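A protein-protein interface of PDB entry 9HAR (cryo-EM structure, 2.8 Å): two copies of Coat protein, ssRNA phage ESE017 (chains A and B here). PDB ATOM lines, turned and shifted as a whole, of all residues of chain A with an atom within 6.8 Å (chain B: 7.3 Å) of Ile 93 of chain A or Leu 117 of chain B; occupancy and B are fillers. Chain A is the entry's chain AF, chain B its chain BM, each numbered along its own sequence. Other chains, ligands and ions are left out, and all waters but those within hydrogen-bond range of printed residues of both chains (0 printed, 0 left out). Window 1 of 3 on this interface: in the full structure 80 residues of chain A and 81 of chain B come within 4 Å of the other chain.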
ATOM      1  N   SER A  71       4.330 -22.371  22.601  1.00  0.00           N
ATOM      2  CA  SER A  71       3.143 -22.466  23.455  1.00  0.00           C
ATOM      3  C   SER A  71       2.242 -23.551  22.876  1.00  0.00           C
ATOM      4  O   SER A  71       1.840 -23.472  21.712  1.00  0.00           O
ATOM      5  CB  SER A  71       2.412 -21.133  23.541  1.00  0.00           C
ATOM      6  OG  SER A  71       2.828 -20.396  24.674  1.00  0.00           O
ATOM      7  N   THR A  72       1.922 -24.554  23.686  1.00  0.00           N
ATOM      8  CA  THR A  72       1.112 -25.672  23.229  1.00  0.00           C
ATOM      9  C   THR A  72      -0.218 -25.734  23.968  1.00  0.00           C
ATOM     10  O   THR A  72      -0.297 -25.487  25.175  1.00  0.00           O
ATOM     11  CB  THR A  72       1.857 -26.994  23.409  1.00  0.00           C
ATOM     12  OG1 THR A  72       3.268 -26.767  23.315  1.00  0.00           O
ATOM     13  CG2 THR A  72       1.439 -27.985  22.340  1.00  0.00           C
ATOM     14  N   VAL A  73      -1.268 -26.068  23.219  1.00  0.00           N
ATOM     15  CA  VAL A  73      -2.597 -26.326  23.762  1.00  0.00           C
ATOM     16  C   VAL A  73      -3.110 -27.632  23.174  1.00  0.00           C
ATOM     17  O   VAL A  73      -3.170 -27.791  21.951  1.00  0.00           O
ATOM     18  CB  VAL A  73      -3.570 -25.175  23.456  1.00  0.00           C
ATOM     19  CG1 VAL A  73      -4.971 -25.559  23.859  1.00  0.00           C
ATOM     20  CG2 VAL A  73      -3.149 -23.920  24.170  1.00  0.00           C
ATOM     21  N   ILE A  74      -3.472 -28.577  24.031  1.00  0.00           N
ATOM     22  CA  ILE A  74      -4.048 -29.841  23.587  1.00  0.00           C
ATOM     23  C   ILE A  74      -5.442 -29.993  24.177  1.00  0.00           C
ATOM     24  O   ILE A  74      -5.610 -30.015  25.398  1.00  0.00           O
ATOM     25  CB  ILE A  74      -3.154 -31.026  23.985  1.00  0.00           C
ATOM     26  CG1 ILE A  74      -1.757 -30.862  23.395  1.00  0.00           C
ATOM     27  CG2 ILE A  74      -3.778 -32.334  23.534  1.00  0.00           C
ATOM     28  CD1 ILE A  74      -0.749 -31.838  23.951  1.00  0.00           C
ATOM     29  N   LEU A  75      -6.441 -30.120  23.313  1.00  0.00           N
ATOM     30  CA  LEU A  75      -7.829 -30.293  23.731  1.00  0.00           C
ATOM     31  C   LEU A  75      -8.175 -31.770  23.564  1.00  0.00           C
ATOM     32  O   LEU A  75      -8.194 -32.297  22.453  1.00  0.00           O
ATOM     33  CB  LEU A  75      -8.758 -29.403  22.922  1.00  0.00           C
ATOM     34  CG  LEU A  75     -10.249 -29.736  22.944  1.00  0.00           C
ATOM     35  CD1 LEU A  75     -10.778 -29.717  24.363  1.00  0.00           C
ATOM     36  CD2 LEU A  75     -11.023 -28.759  22.077  1.00  0.00           C
ATOM     37  N   VAL A  91      -6.980 -32.308  19.771  1.00  0.00           N
ATOM     38  CA  VAL A  91      -6.642 -31.187  18.901  1.00  0.00           C
ATOM     39  C   VAL A  91      -5.474 -30.423  19.509  1.00  0.00           C
ATOM     40  O   VAL A  91      -5.661 -29.606  20.416  1.00  0.00           O
ATOM     41  CB  VAL A  91      -7.841 -30.247  18.686  1.00  0.00           C
ATOM     42  CG1 VAL A  91      -7.444 -29.105  17.774  1.00  0.00           C
ATOM     43  CG2 VAL A  91      -9.021 -31.000  18.121  1.00  0.00           C
ATOM     44  N   SER A  92      -4.265 -30.680  19.022  1.00  0.00           N
ATOM     45  CA  SER A  92      -3.101 -29.974  19.533  1.00  0.00           C
ATOM     46  C   SER A  92      -2.794 -28.747  18.681  1.00  0.00           C
ATOM     47  O   SER A  92      -3.008 -28.735  17.468  1.00  0.00           O
ATOM     48  CB  SER A  92      -1.887 -30.899  19.570  1.00  0.00           C
ATOM     49  OG  SER A  92      -1.747 -31.604  18.351  1.00  0.00           O
ATOM     50  N   ILE A  93      -2.293 -27.702  19.340  1.00  0.00           N
ATOM     51  CA  ILE A  93      -1.935 -26.452  18.680  1.00  0.00           C
ATOM     52  C   ILE A  93      -0.626 -25.943  19.269  1.00  0.00           C
ATOM     53  O   ILE A  93      -0.471 -25.885  20.492  1.00  0.00           O
ATOM     54  CB  ILE A  93      -3.050 -25.404  18.835  1.00  0.00           C
ATOM     55  CG1 ILE A  93      -4.333 -25.886  18.157  1.00  0.00           C
ATOM     56  CG2 ILE A  93      -2.610 -24.083  18.251  1.00  0.00           C
ATOM     57  CD1 ILE A  93      -5.451 -24.889  18.175  1.00  0.00           C
ATOM     58  N   GLN A  94       0.323 -25.577  18.415  1.00  0.00           N
ATOM     59  CA  GLN A  94       1.620 -25.083  18.856  1.00  0.00           C
ATOM     60  C   GLN A  94       1.939 -23.758  18.174  1.00  0.00           C
ATOM     61  O   GLN A  94       1.504 -23.499  17.049  1.00  0.00           O
ATOM     62  CB  GLN A  94       2.721 -26.109  18.575  1.00  0.00           C
ATOM     63  CG  GLN A  94       3.991 -25.879  19.373  1.00  0.00           C
ATOM     64  CD  GLN A  94       4.991 -27.011  19.233  1.00  0.00           C
ATOM     65  OE1 GLN A  94       4.847 -28.060  19.858  1.00  0.00           O
ATOM     66  NE2 GLN A  94       6.009 -26.802  18.410  1.00  0.00           N
ATOM     67  N   LEU A  95       2.697 -22.912  18.875  1.00  0.00           N
ATOM     68  CA  LEU A  95       2.974 -21.540  18.448  1.00  0.00           C
ATOM     69  C   LEU A  95       4.476 -21.247  18.562  1.00  0.00           C
ATOM     70  O   LEU A  95       4.910 -20.323  19.244  1.00  0.00           O
ATOM     71  CB  LEU A  95       2.147 -20.536  19.245  1.00  0.00           C
ATOM     72  CG  LEU A  95       2.273 -19.062  18.842  1.00  0.00           C
ATOM     73  CD1 LEU A  95       1.336 -18.708  17.709  1.00  0.00           C
ATOM     74  CD2 LEU A  95       2.043 -18.164  20.024  1.00  0.00           C
ATOM     75  N   VAL A 106       1.963 -11.757  16.106  1.00  0.00           N
ATOM     76  CA  VAL A 106       1.443 -12.944  16.780  1.00  0.00           C
ATOM     77  C   VAL A 106      -0.076 -12.975  16.698  1.00  0.00           C
ATOM     78  O   VAL A 106      -0.676 -14.023  16.440  1.00  0.00           O
ATOM     79  CB  VAL A 106       1.934 -12.992  18.239  1.00  0.00           C
ATOM     80  CG1 VAL A 106       1.083 -13.945  19.055  1.00  0.00           C
ATOM     81  CG2 VAL A 106       3.388 -13.403  18.292  1.00  0.00           C
ATOM     82  N   THR A 107      -0.723 -11.827  16.914  1.00  0.00           N
ATOM     83  CA  THR A 107      -2.174 -11.755  16.776  1.00  0.00           C
ATOM     84  C   THR A 107      -2.607 -12.059  15.349  1.00  0.00           C
ATOM     85  O   THR A 107      -3.602 -12.759  15.129  1.00  0.00           O
ATOM     86  CB  THR A 107      -2.671 -10.374  17.202  1.00  0.00           C
ATOM     87  OG1 THR A 107      -2.242 -10.103  18.541  1.00  0.00           O
ATOM     88  CG2 THR A 107      -4.186 -10.309  17.141  1.00  0.00           C
ATOM     89  N   MET A 109      -1.038 -13.956  13.184  1.00  0.00           N
ATOM     90  CA  MET A 109      -0.851 -15.386  12.979  1.00  0.00           C
ATOM     91  C   MET A 109      -1.947 -16.190  13.664  1.00  0.00           C
ATOM     92  O   MET A 109      -2.449 -17.175  13.115  1.00  0.00           O
ATOM     93  CB  MET A 109       0.524 -15.796  13.496  1.00  0.00           C
ATOM     94  CG  MET A 109       1.562 -15.960  12.411  1.00  0.00           C
ATOM     95  SD  MET A 109       2.867 -17.066  12.946  1.00  0.00           S
ATOM     96  CE  MET A 109       3.072 -16.467  14.612  1.00  0.00           C
ATOM     97  N   LEU A 110      -2.318 -15.795  14.882  1.00  0.00           N
ATOM     98  CA  LEU A 110      -3.351 -16.517  15.612  1.00  0.00           C
ATOM     99  C   LEU A 110      -4.698 -16.385  14.915  1.00  0.00           C
ATOM    100  O   LEU A 110      -5.481 -17.338  14.865  1.00  0.00           O
ATOM    101  CB  LEU A 110      -3.434 -16.010  17.052  1.00  0.00           C
ATOM    102  CG  LEU A 110      -2.259 -16.297  17.992  1.00  0.00           C
ATOM    103  CD1 LEU A 110      -2.347 -15.413  19.224  1.00  0.00           C
ATOM    104  CD2 LEU A 110      -2.203 -17.756  18.392  1.00  0.00           C
ATOM    105  N   ASN A 111      -4.991 -15.198  14.377  1.00  0.00           N
ATOM    106  CA  ASN A 111      -6.224 -15.020  13.619  1.00  0.00           C
ATOM    107  C   ASN A 111      -6.211 -15.846  12.339  1.00  0.00           C
ATOM    108  O   ASN A 111      -7.221 -16.460  11.981  1.00  0.00           O
ATOM    109  CB  ASN A 111      -6.443 -13.544  13.296  1.00  0.00           C
ATOM    110  CG  ASN A 111      -7.641 -13.326  12.402  1.00  0.00           C
ATOM    111  OD1 ASN A 111      -8.784 -13.402  12.847  1.00  0.00           O
ATOM    112  ND2 ASN A 111      -7.386 -13.063  11.126  1.00  0.00           N
ATOM    113  N   ALA A 113      -4.479 -18.642  11.681  1.00  0.00           N
ATOM    114  CA  ALA A 113      -4.608 -20.042  12.063  1.00  0.00           C
ATOM    115  C   ALA A 113      -6.000 -20.393  12.561  1.00  0.00           C
ATOM    116  O   ALA A 113      -6.533 -21.446  12.196  1.00  0.00           O
ATOM    117  CB  ALA A 113      -3.587 -20.390  13.144  1.00  0.00           C
ATOM    118  N   ALA A 114      -6.598 -19.541  13.392  1.00  0.00           N
ATOM    119  CA  ALA A 114      -7.950 -19.785  13.867  1.00  0.00           C
ATOM    120  C   ALA A 114      -8.995 -19.482  12.811  1.00  0.00           C
ATOM    121  O   ALA A 114     -10.150 -19.871  12.982  1.00  0.00           O
ATOM    122  CB  ALA A 114      -8.231 -18.962  15.122  1.00  0.00           C
ATOM    123  N   GLN A 115      -8.624 -18.787  11.736  1.00  0.00           N
ATOM    124  CA  GLN A 115      -9.518 -18.646  10.596  1.00  0.00           C
ATOM    125  C   GLN A 115      -9.708 -19.966   9.870  1.00  0.00           C
ATOM    126  O   GLN A 115     -10.773 -20.196   9.290  1.00  0.00           O
ATOM    127  CB  GLN A 115      -8.980 -17.594   9.633  1.00  0.00           C
ATOM    128  CG  GLN A 115      -9.987 -17.102   8.626  1.00  0.00           C
ATOM    129  CD  GLN A 115     -10.072 -15.600   8.617  1.00  0.00           C
ATOM    130  OE1 GLN A 115      -9.163 -14.920   9.085  1.00  0.00           O
ATOM    131  NE2 GLN A 115     -11.160 -15.068   8.079  1.00  0.00           N
ATOM    132  N   LEU A 116      -8.696 -20.825   9.884  1.00  0.00           N
ATOM    133  CA  LEU A 116      -8.878 -22.237   9.618  1.00  0.00           C
ATOM    134  C   LEU A 116      -9.644 -22.846  10.794  1.00  0.00           C
ATOM    135  O   LEU A 116      -9.874 -22.195  11.815  1.00  0.00           O
ATOM    136  CB  LEU A 116      -7.524 -22.912   9.408  1.00  0.00           C
ATOM    137  CG  LEU A 116      -6.590 -22.269   8.379  1.00  0.00           C
ATOM    138  CD1 LEU A 116      -5.150 -22.263   8.873  1.00  0.00           C
ATOM    139  CD2 LEU A 116      -6.686 -22.970   7.038  1.00  0.00           C
ATOM    140  N   LEU A 117     -10.059 -24.101  10.646  1.00  0.00           N
ATOM    141  CA  LEU A 117     -10.795 -24.846  11.675  1.00  0.00           C
ATOM    142  C   LEU A 117     -12.243 -24.378  11.826  1.00  0.00           C
ATOM    143  O   LEU A 117     -13.036 -25.029  12.507  1.00  0.00           O
ATOM    144  CB  LEU A 117     -10.110 -24.784  13.047  1.00  0.00           C
ATOM    145  CG  LEU A 117      -8.609 -24.945  13.261  1.00  0.00           C
ATOM    146  CD1 LEU A 117      -8.200 -24.193  14.505  1.00  0.00           C
ATOM    147  CD2 LEU A 117      -8.288 -26.399  13.428  1.00  0.00           C
ATOM    148  N   VAL B  91       2.745 -22.036  13.169  1.00  0.00           N
ATOM    149  CA  VAL B  91       1.566 -22.407  13.943  1.00  0.00           C
ATOM    150  C   VAL B  91       1.030 -23.729  13.414  1.00  0.00           C
ATOM    151  O   VAL B  91       0.332 -23.764  12.396  1.00  0.00           O
ATOM    152  CB  VAL B  91       0.476 -21.322  13.880  1.00  0.00           C
ATOM    153  CG1 VAL B  91      -0.717 -21.739  14.715  1.00  0.00           C
ATOM    154  CG2 VAL B  91       1.017 -19.981  14.335  1.00  0.00           C
ATOM    155  N   SER B  92       1.351 -24.825  14.091  1.00  0.00           N
ATOM    156  CA  SER B  92       0.889 -26.130  13.648  1.00  0.00           C
ATOM    157  C   SER B  92      -0.385 -26.534  14.382  1.00  0.00           C
ATOM    158  O   SER B  92      -0.595 -26.190  15.546  1.00  0.00           O
ATOM    159  CB  SER B  92       1.972 -27.184  13.866  1.00  0.00           C
ATOM    160  OG  SER B  92       2.530 -27.078  15.160  1.00  0.00           O
ATOM    161  N   ILE B  93      -1.244 -27.271  13.680  1.00  0.00           N
ATOM    162  CA  ILE B  93      -2.508 -27.748  14.230  1.00  0.00           C
ATOM    163  C   ILE B  93      -2.728 -29.184  13.773  1.00  0.00           C
ATOM    164  O   ILE B  93      -2.593 -29.489  12.585  1.00  0.00           O
ATOM    165  CB  ILE B  93      -3.677 -26.847  13.797  1.00  0.00           C
ATOM    166  CG1 ILE B  93      -3.479 -25.424  14.323  1.00  0.00           C
ATOM    167  CG2 ILE B  93      -4.986 -27.411  14.295  1.00  0.00           C
ATOM    168  CD1 ILE B  93      -4.607 -24.488  13.996  1.00  0.00           C
ATOM    169  N   GLN B  94      -3.063 -30.074  14.700  1.00  0.00           N
ATOM    170  CA  GLN B  94      -3.312 -31.472  14.382  1.00  0.00           C
ATOM    171  C   GLN B  94      -4.657 -31.912  14.948  1.00  0.00           C
ATOM    172  O   GLN B  94      -5.140 -31.363  15.941  1.00  0.00           O
ATOM    173  CB  GLN B  94      -2.189 -32.366  14.913  1.00  0.00           C
ATOM    174  CG  GLN B  94      -2.156 -33.746  14.276  1.00  0.00           C
ATOM    175  CD  GLN B  94      -0.923 -34.545  14.653  1.00  0.00           C
ATOM    176  OE1 GLN B  94       0.156 -34.336  14.103  1.00  0.00           O
ATOM    177  NE2 GLN B  94      -1.081 -35.466  15.593  1.00  0.00           N
ATOM    178  N   LEU B 110     -13.485 -28.457  16.572  1.00  0.00           N
ATOM    179  CA  LEU B 110     -12.813 -27.419  15.800  1.00  0.00           C
ATOM    180  C   LEU B 110     -13.223 -26.036  16.280  1.00  0.00           C
ATOM    181  O   LEU B 110     -12.401 -25.119  16.344  1.00  0.00           O
ATOM    182  CB  LEU B 110     -13.124 -27.588  14.313  1.00  0.00           C
ATOM    183  CG  LEU B 110     -12.535 -28.787  13.567  1.00  0.00           C
ATOM    184  CD1 LEU B 110     -13.251 -28.970  12.240  1.00  0.00           C
ATOM    185  CD2 LEU B 110     -11.044 -28.648  13.354  1.00  0.00           C
ATOM    186  N   ALA B 112     -14.294 -25.316  19.372  1.00  0.00           N
ATOM    187  CA  ALA B 112     -13.726 -25.121  20.700  1.00  0.00           C
ATOM    188  C   ALA B 112     -12.241 -24.792  20.627  1.00  0.00           C
ATOM    189  O   ALA B 112     -11.773 -23.867  21.301  1.00  0.00           O
ATOM    190  CB  ALA B 112     -13.961 -26.364  21.558  1.00  0.00           C
ATOM    191  N   ALA B 113     -11.485 -25.534  19.816  1.00  0.00           N
ATOM    192  CA  ALA B 113     -10.069 -25.257  19.617  1.00  0.00           C
ATOM    193  C   ALA B 113      -9.820 -23.907  18.966  1.00  0.00           C
ATOM    194  O   ALA B 113      -8.927 -23.173  19.401  1.00  0.00           O
ATOM    195  CB  ALA B 113      -9.433 -26.351  18.761  1.00  0.00           C
ATOM    196  N   ALA B 114     -10.584 -23.566  17.932  1.00  0.00           N
ATOM    197  CA  ALA B 114     -10.448 -22.266  17.299  1.00  0.00           C
ATOM    198  C   ALA B 114     -11.049 -21.154  18.137  1.00  0.00           C
ATOM    199  O   ALA B 114     -10.790 -19.985  17.854  1.00  0.00           O
ATOM    200  CB  ALA B 114     -11.097 -22.275  15.916  1.00  0.00           C
ATOM    201  N   GLN B 115     -11.860 -21.488  19.141  1.00  0.00           N
ATOM    202  CA  GLN B 115     -12.318 -20.489  20.097  1.00  0.00           C
ATOM    203  C   GLN B 115     -11.184 -19.999  20.978  1.00  0.00           C
ATOM    204  O   GLN B 115     -11.213 -18.853  21.435  1.00  0.00           O
ATOM    205  CB  GLN B 115     -13.437 -21.066  20.957  1.00  0.00           C
ATOM    206  CG  GLN B 115     -14.066 -20.087  21.904  1.00  0.00           C
ATOM    207  CD  GLN B 115     -15.552 -20.002  21.694  1.00  0.00           C
ATOM    208  OE1 GLN B 115     -16.163 -20.936  21.183  1.00  0.00           O
ATOM    209  NE2 GLN B 115     -16.146 -18.886  22.089  1.00  0.00           N
ATOM    210  N   LEU B 116     -10.194 -20.848  21.226  1.00  0.00           N
ATOM    211  CA  LEU B 116      -8.885 -20.415  21.672  1.00  0.00           C
ATOM    212  C   LEU B 116      -8.211 -19.669  20.518  1.00  0.00           C
ATOM    213  O   LEU B 116      -8.757 -19.556  19.419  1.00  0.00           O
ATOM    214  CB  LEU B 116      -8.060 -21.616  22.126  1.00  0.00           C
ATOM    215  CG  LEU B 116      -8.680 -22.536  23.183  1.00  0.00           C
ATOM    216  CD1 LEU B 116      -8.396 -23.996  22.863  1.00  0.00           C
ATOM    217  CD2 LEU B 116      -8.174 -22.201  24.571  1.00  0.00           C
ATOM    218  N   LEU B 117      -7.022 -19.132  20.770  1.00  0.00           N
ATOM    219  CA  LEU B 117      -6.217 -18.436  19.760  1.00  0.00           C
ATOM    220  C   LEU B 117      -6.815 -17.094  19.340  1.00  0.00           C
ATOM    221  O   LEU B 117      -6.165 -16.322  18.635  1.00  0.00           O
ATOM    222  CB  LEU B 117      -6.001 -19.292  18.507  1.00  0.00           C
ATOM    223  CG  LEU B 117      -5.530 -20.742  18.528  1.00  0.00           C
ATOM    224  CD1 LEU B 117      -6.201 -21.481  17.393  1.00  0.00           C
ATOM    225  CD2 LEU B 117      -4.039 -20.794  18.353  1.00  0.00           C
ATOM    226  N   PHE B 118      -8.043 -16.773  19.748  1.00  0.00           N
ATOM    227  CA  PHE B 118      -8.506 -15.408  19.528  1.00  0.00           C
ATOM    228  C   PHE B 118      -9.310 -14.902  20.715  1.00  0.00           C
ATOM    229  O   PHE B 118      -9.709 -13.734  20.745  1.00  0.00           O
ATOM    230  CB  PHE B 118      -9.309 -15.281  18.220  1.00  0.00           C
ATOM    231  CG  PHE B 118     -10.720 -15.820  18.281  1.00  0.00           C
ATOM    232  CD1 PHE B 118     -11.747 -15.088  18.858  1.00  0.00           C
ATOM    233  CD2 PHE B 118     -11.030 -17.024  17.690  1.00  0.00           C
ATOM    234  CE1 PHE B 118     -13.034 -15.579  18.892  1.00  0.00           C
ATOM    235  CE2 PHE B 118     -12.320 -17.512  17.712  1.00  0.00           C
ATOM    236  CZ  PHE B 118     -13.318 -16.793  18.314  1.00  0.00           C
ATOM    237  N   ASP B 119      -9.550 -15.765  21.694  1.00  0.00           N
ATOM    238  CA  ASP B 119     -10.210 -15.316  22.905  1.00  0.00           C
ATOM    239  C   ASP B 119      -9.256 -14.443  23.711  1.00  0.00           C
ATOM    240  O   ASP B 119      -8.056 -14.710  23.805  1.00  0.00           O
ATOM    241  CB  ASP B 119     -10.685 -16.507  23.736  1.00  0.00           C
ATOM    242  CG  ASP B 119     -11.835 -16.156  24.657  1.00  0.00           C
ATOM    243  OD1 ASP B 119     -11.823 -15.049  25.233  1.00  0.00           O
ATOM    244  OD2 ASP B 119     -12.755 -16.985  24.804  1.00  0.00           O
ATOM    245  N   SER B 120      -9.806 -13.381  24.293  1.00  0.00           N
ATOM    246  CA  SER B 120      -8.996 -12.422  25.029  1.00  0.00           C
ATOM    247  C   SER B 120      -8.338 -13.020  26.262  1.00  0.00           C
ATOM    248  O   SER B 120      -7.300 -12.511  26.698  1.00  0.00           O
ATOM    249  CB  SER B 120      -9.849 -11.221  25.447  1.00  0.00           C
ATOM    250  OG  SER B 120     -10.665 -11.548  26.556  1.00  0.00           O
ATOM    251  N   TYR B 122      -6.766 -15.832  26.570  1.00  0.00           N
ATOM    252  CA  TYR B 122      -5.539 -16.534  26.234  1.00  0.00           C
ATOM    253  C   TYR B 122      -4.517 -15.653  25.530  1.00  0.00           C
ATOM    254  O   TYR B 122      -3.469 -16.159  25.117  1.00  0.00           O
ATOM    255  CB  TYR B 122      -5.876 -17.754  25.376  1.00  0.00           C
ATOM    256  CG  TYR B 122      -7.043 -18.533  25.934  1.00  0.00           C
ATOM    257  CD1 TYR B 122      -6.918 -19.257  27.112  1.00  0.00           C
ATOM    258  CD2 TYR B 122      -8.281 -18.511  25.310  1.00  0.00           C
ATOM    259  CE1 TYR B 122      -7.981 -19.958  27.635  1.00  0.00           C
ATOM    260  CE2 TYR B 122      -9.354 -19.206  25.830  1.00  0.00           C
ATOM    261  CZ  TYR B 122      -9.197 -19.927  26.992  1.00  0.00           C
ATOM    262  OH  TYR B 122     -10.261 -20.625  27.511  1.00  0.00           O
ATOM    263  N   SER B 123      -4.791 -14.355  25.393  1.00  0.00           N
ATOM    264  CA  SER B 123      -3.857 -13.433  24.756  1.00  0.00           C
ATOM    265  C   SER B 123      -2.481 -13.477  25.411  1.00  0.00           C
ATOM    266  O   SER B 123      -1.456 -13.598  24.731  1.00  0.00           O
ATOM    267  CB  SER B 123      -4.423 -12.011  24.801  1.00  0.00           C
ATOM    268  OG  SER B 123      -5.352 -11.792  23.756  1.00  0.00           O
ATOM    269  N   PHE B 125      -1.273 -15.822  27.337  1.00  0.00           N
ATOM    270  CA  PHE B 125      -0.689 -17.149  27.178  1.00  0.00           C
ATOM    271  C   PHE B 125       0.004 -17.287  25.829  1.00  0.00           C
ATOM    272  O   PHE B 125       1.124 -17.803  25.736  1.00  0.00           O
ATOM    273  CB  PHE B 125      -1.759 -18.225  27.332  1.00  0.00           C
ATOM    274  CG  PHE B 125      -1.258 -19.599  27.027  1.00  0.00           C
ATOM    275  CD1 PHE B 125      -0.315 -20.200  27.835  1.00  0.00           C
ATOM    276  CD2 PHE B 125      -1.695 -20.269  25.902  1.00  0.00           C
ATOM    277  CE1 PHE B 125       0.155 -21.456  27.543  1.00  0.00           C
ATOM    278  CE2 PHE B 125      -1.223 -21.515  25.607  1.00  0.00           C
ATOM    279  CZ  PHE B 125      -0.298 -22.115  26.427  1.00  0.00           C
ATOM    280  N   TRP B 126      -0.656 -16.840  24.762  1.00  0.00           N
ATOM    281  CA  TRP B 126      -0.068 -16.958  23.437  1.00  0.00           C
ATOM    282  C   TRP B 126       1.068 -15.971  23.216  1.00  0.00           C
ATOM    283  O   TRP B 126       1.989 -16.277  22.455  1.00  0.00           O
ATOM    284  CB  TRP B 126      -1.145 -16.759  22.368  1.00  0.00           C
ATOM    285  CG  TRP B 126      -2.092 -17.911  22.234  1.00  0.00           C
ATOM    286  CD1 TRP B 126      -3.443 -17.872  22.379  1.00  0.00           C
ATOM    287  CD2 TRP B 126      -1.763 -19.268  21.913  1.00  0.00           C
ATOM    288  NE1 TRP B 126      -3.979 -19.118  22.182  1.00  0.00           N
ATOM    289  CE2 TRP B 126      -2.967 -19.993  21.893  1.00  0.00           C
ATOM    290  CE3 TRP B 126      -0.569 -19.938  21.646  1.00  0.00           C
ATOM    291  CZ2 TRP B 126      -3.012 -21.353  21.616  1.00  0.00           C
ATOM    292  CZ3 TRP B 126      -0.616 -21.287  21.371  1.00  0.00           C
ATOM    293  CH2 TRP B 126      -1.829 -21.981  21.358  1.00  0.00           C
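The backbone NH of Ile 93 of chain A is in hydrogen-bond range of the backbone carbonyl oxygen of Val 73 of chain A (2.8 Å).
O of Ser 71 of chain A sits at hydrogen-bond distance from N of Leu 95 of chain A.
O of Leu 75 of chain A is in hydrogen-bond range of N of Val 91 of chain A.
Of chain B, only Ser 92, Ile 93, Leu 117 and Trp 126 come within 4 Å of Ile 93 of chain A.
Printed residues of chain A within 4 Å of Leu 117 of chain B: Ile 93, Leu 110 and Ala 114.
Printed residues of chain B within 4 Å of Gln 94 of chain A: Val 91 (3.3 Å) and Ser 92 (3.1 Å).
Of the printed residues of chain B, Thr 72 of chain A touches Phe 125.
Printed residues of chain B within 4 Å of Val 73 of chain A: Leu 116 (3.9 Å), Phe 125 (3.4 Å) and Trp 126 (3.6 Å).
Gln 115 of chain A touches none of the printed residues of chain B.
The nearest residue of chain A that does not touch Leu 117 of chain B is Leu 117 of chain A (4.4 Å).
OG of Ser 71 of chain A sits at hydrogen-bond distance from O of Phe 125 of chain B.
O of Ser 92 of chain B sits at hydrogen-bond distance from N of Gln 94 of chain A (3.1 Å).
The backbone carbonyl oxygen (O) of Ser 92 of chain A lies within hydrogen-bond range of the backbone NH (N) of Gln 94 of chain B.
Of the 20 printed residues of chain A, 14 touch a printed residue of chain B.
Hydrophobic or aromatic side chains of chain A that line the printed part of chain B: Val 73, Leu 75, Val 91, Ile 93, Leu 95, Met 109, Leu 110, Ala 113, Ala 114 and Leu 117.
Printed residues of chain B that touch a printed residue of chain A: Val 91, Ser 92, Ile 93, Gln 94, Leu 110, Ala 112, Ala 113, Ala 114, Leu 116, Leu 117, Phe 125 and Trp 126.
Hydrophobic or aromatic side chains of chain B that line the printed part of chain A: Val 91, Ile 93, Leu 110, Ala 112, Ala 113, Ala 114, Leu 116, Leu 117, Phe 125 and Trp 126.
Along chain B the printed residues that touch a printed residue of chain A span positions 91 to 126.
Among the printed residues, no Asp or Glu carboxylate lies within 4 Å of a Lys or Arg side-chain nitrogen of the other chain.
Among the printed residues, merely in contact across the chains: Leu 95 of chain A with Trp 126 of chain B, Leu 117 of chain A with Leu 110 of chain B, Leu 110 of chain A with Leu 117 of chain B, Gln 94 of chain A with Val 91 of chain B, Ser 71 of chain A with Trp 126 of chain B, Val 91 of chain A with Gln 94 of chain B, Val 73 of chain A with Phe 125 of chain B, Ile 93 of chain A with Ser 92 of chain B, Ser 92 of chain A with Ile 93 of chain B, Val 91 of chain A with Ala 113 of chain B, Ala 113 of chain A with Val 91 of chain B, Leu 117 of chain A with Ile 93 of chain B, Ile 93 of chain A with Leu 117 of chain B, Thr 72 of chain A with Phe 125 of chain B, Leu 95 of chain A with Val 91 of chain B, Val 73 of chain A with Trp 126 of chain B, Leu 110 of chain A with Trp 126 of chain B, Met 109 of chain A with Val 91 of chain B, Leu 117 of chain A with Ala 114 of chain B, Leu 75 of chain A with Ala 112 of chain B, Ile 93 of chain A with Trp 126 of chain B, Ala 114 of chain A with Ala 114 of chain B, Val 73 of chain A with Leu 116 of chain B, Ala 114 of chain A with Leu 117 of chain B, Ile 93 of chain A with Ile 93 of chain B, Leu 75 of chain A with Ala 113 of chain B and Ser 92 of chain A with Ser 92 of chain B.
Val 91 of chain A touches Gln 94 of chain B, and with the chains exchanged Gln 94 of chain A touches Val 91 of chain B.
Ser 92 of chain A touches Gln 94 of chain B, and with the chains exchanged Gln 94 of chain A touches Ser 92 of chain B.
Ala 114 of chain B touches its own counterpart, Ala 114 of chain A.
Ala 114 of chain A touches Leu 117 of chain B, and with the chains exchanged Leu 117 of chain A touches Ala 114 of chain B.
Of the 30 pairs that touch across the chains among the printed residues, 17 have their exchanged pair printed and touching as well.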
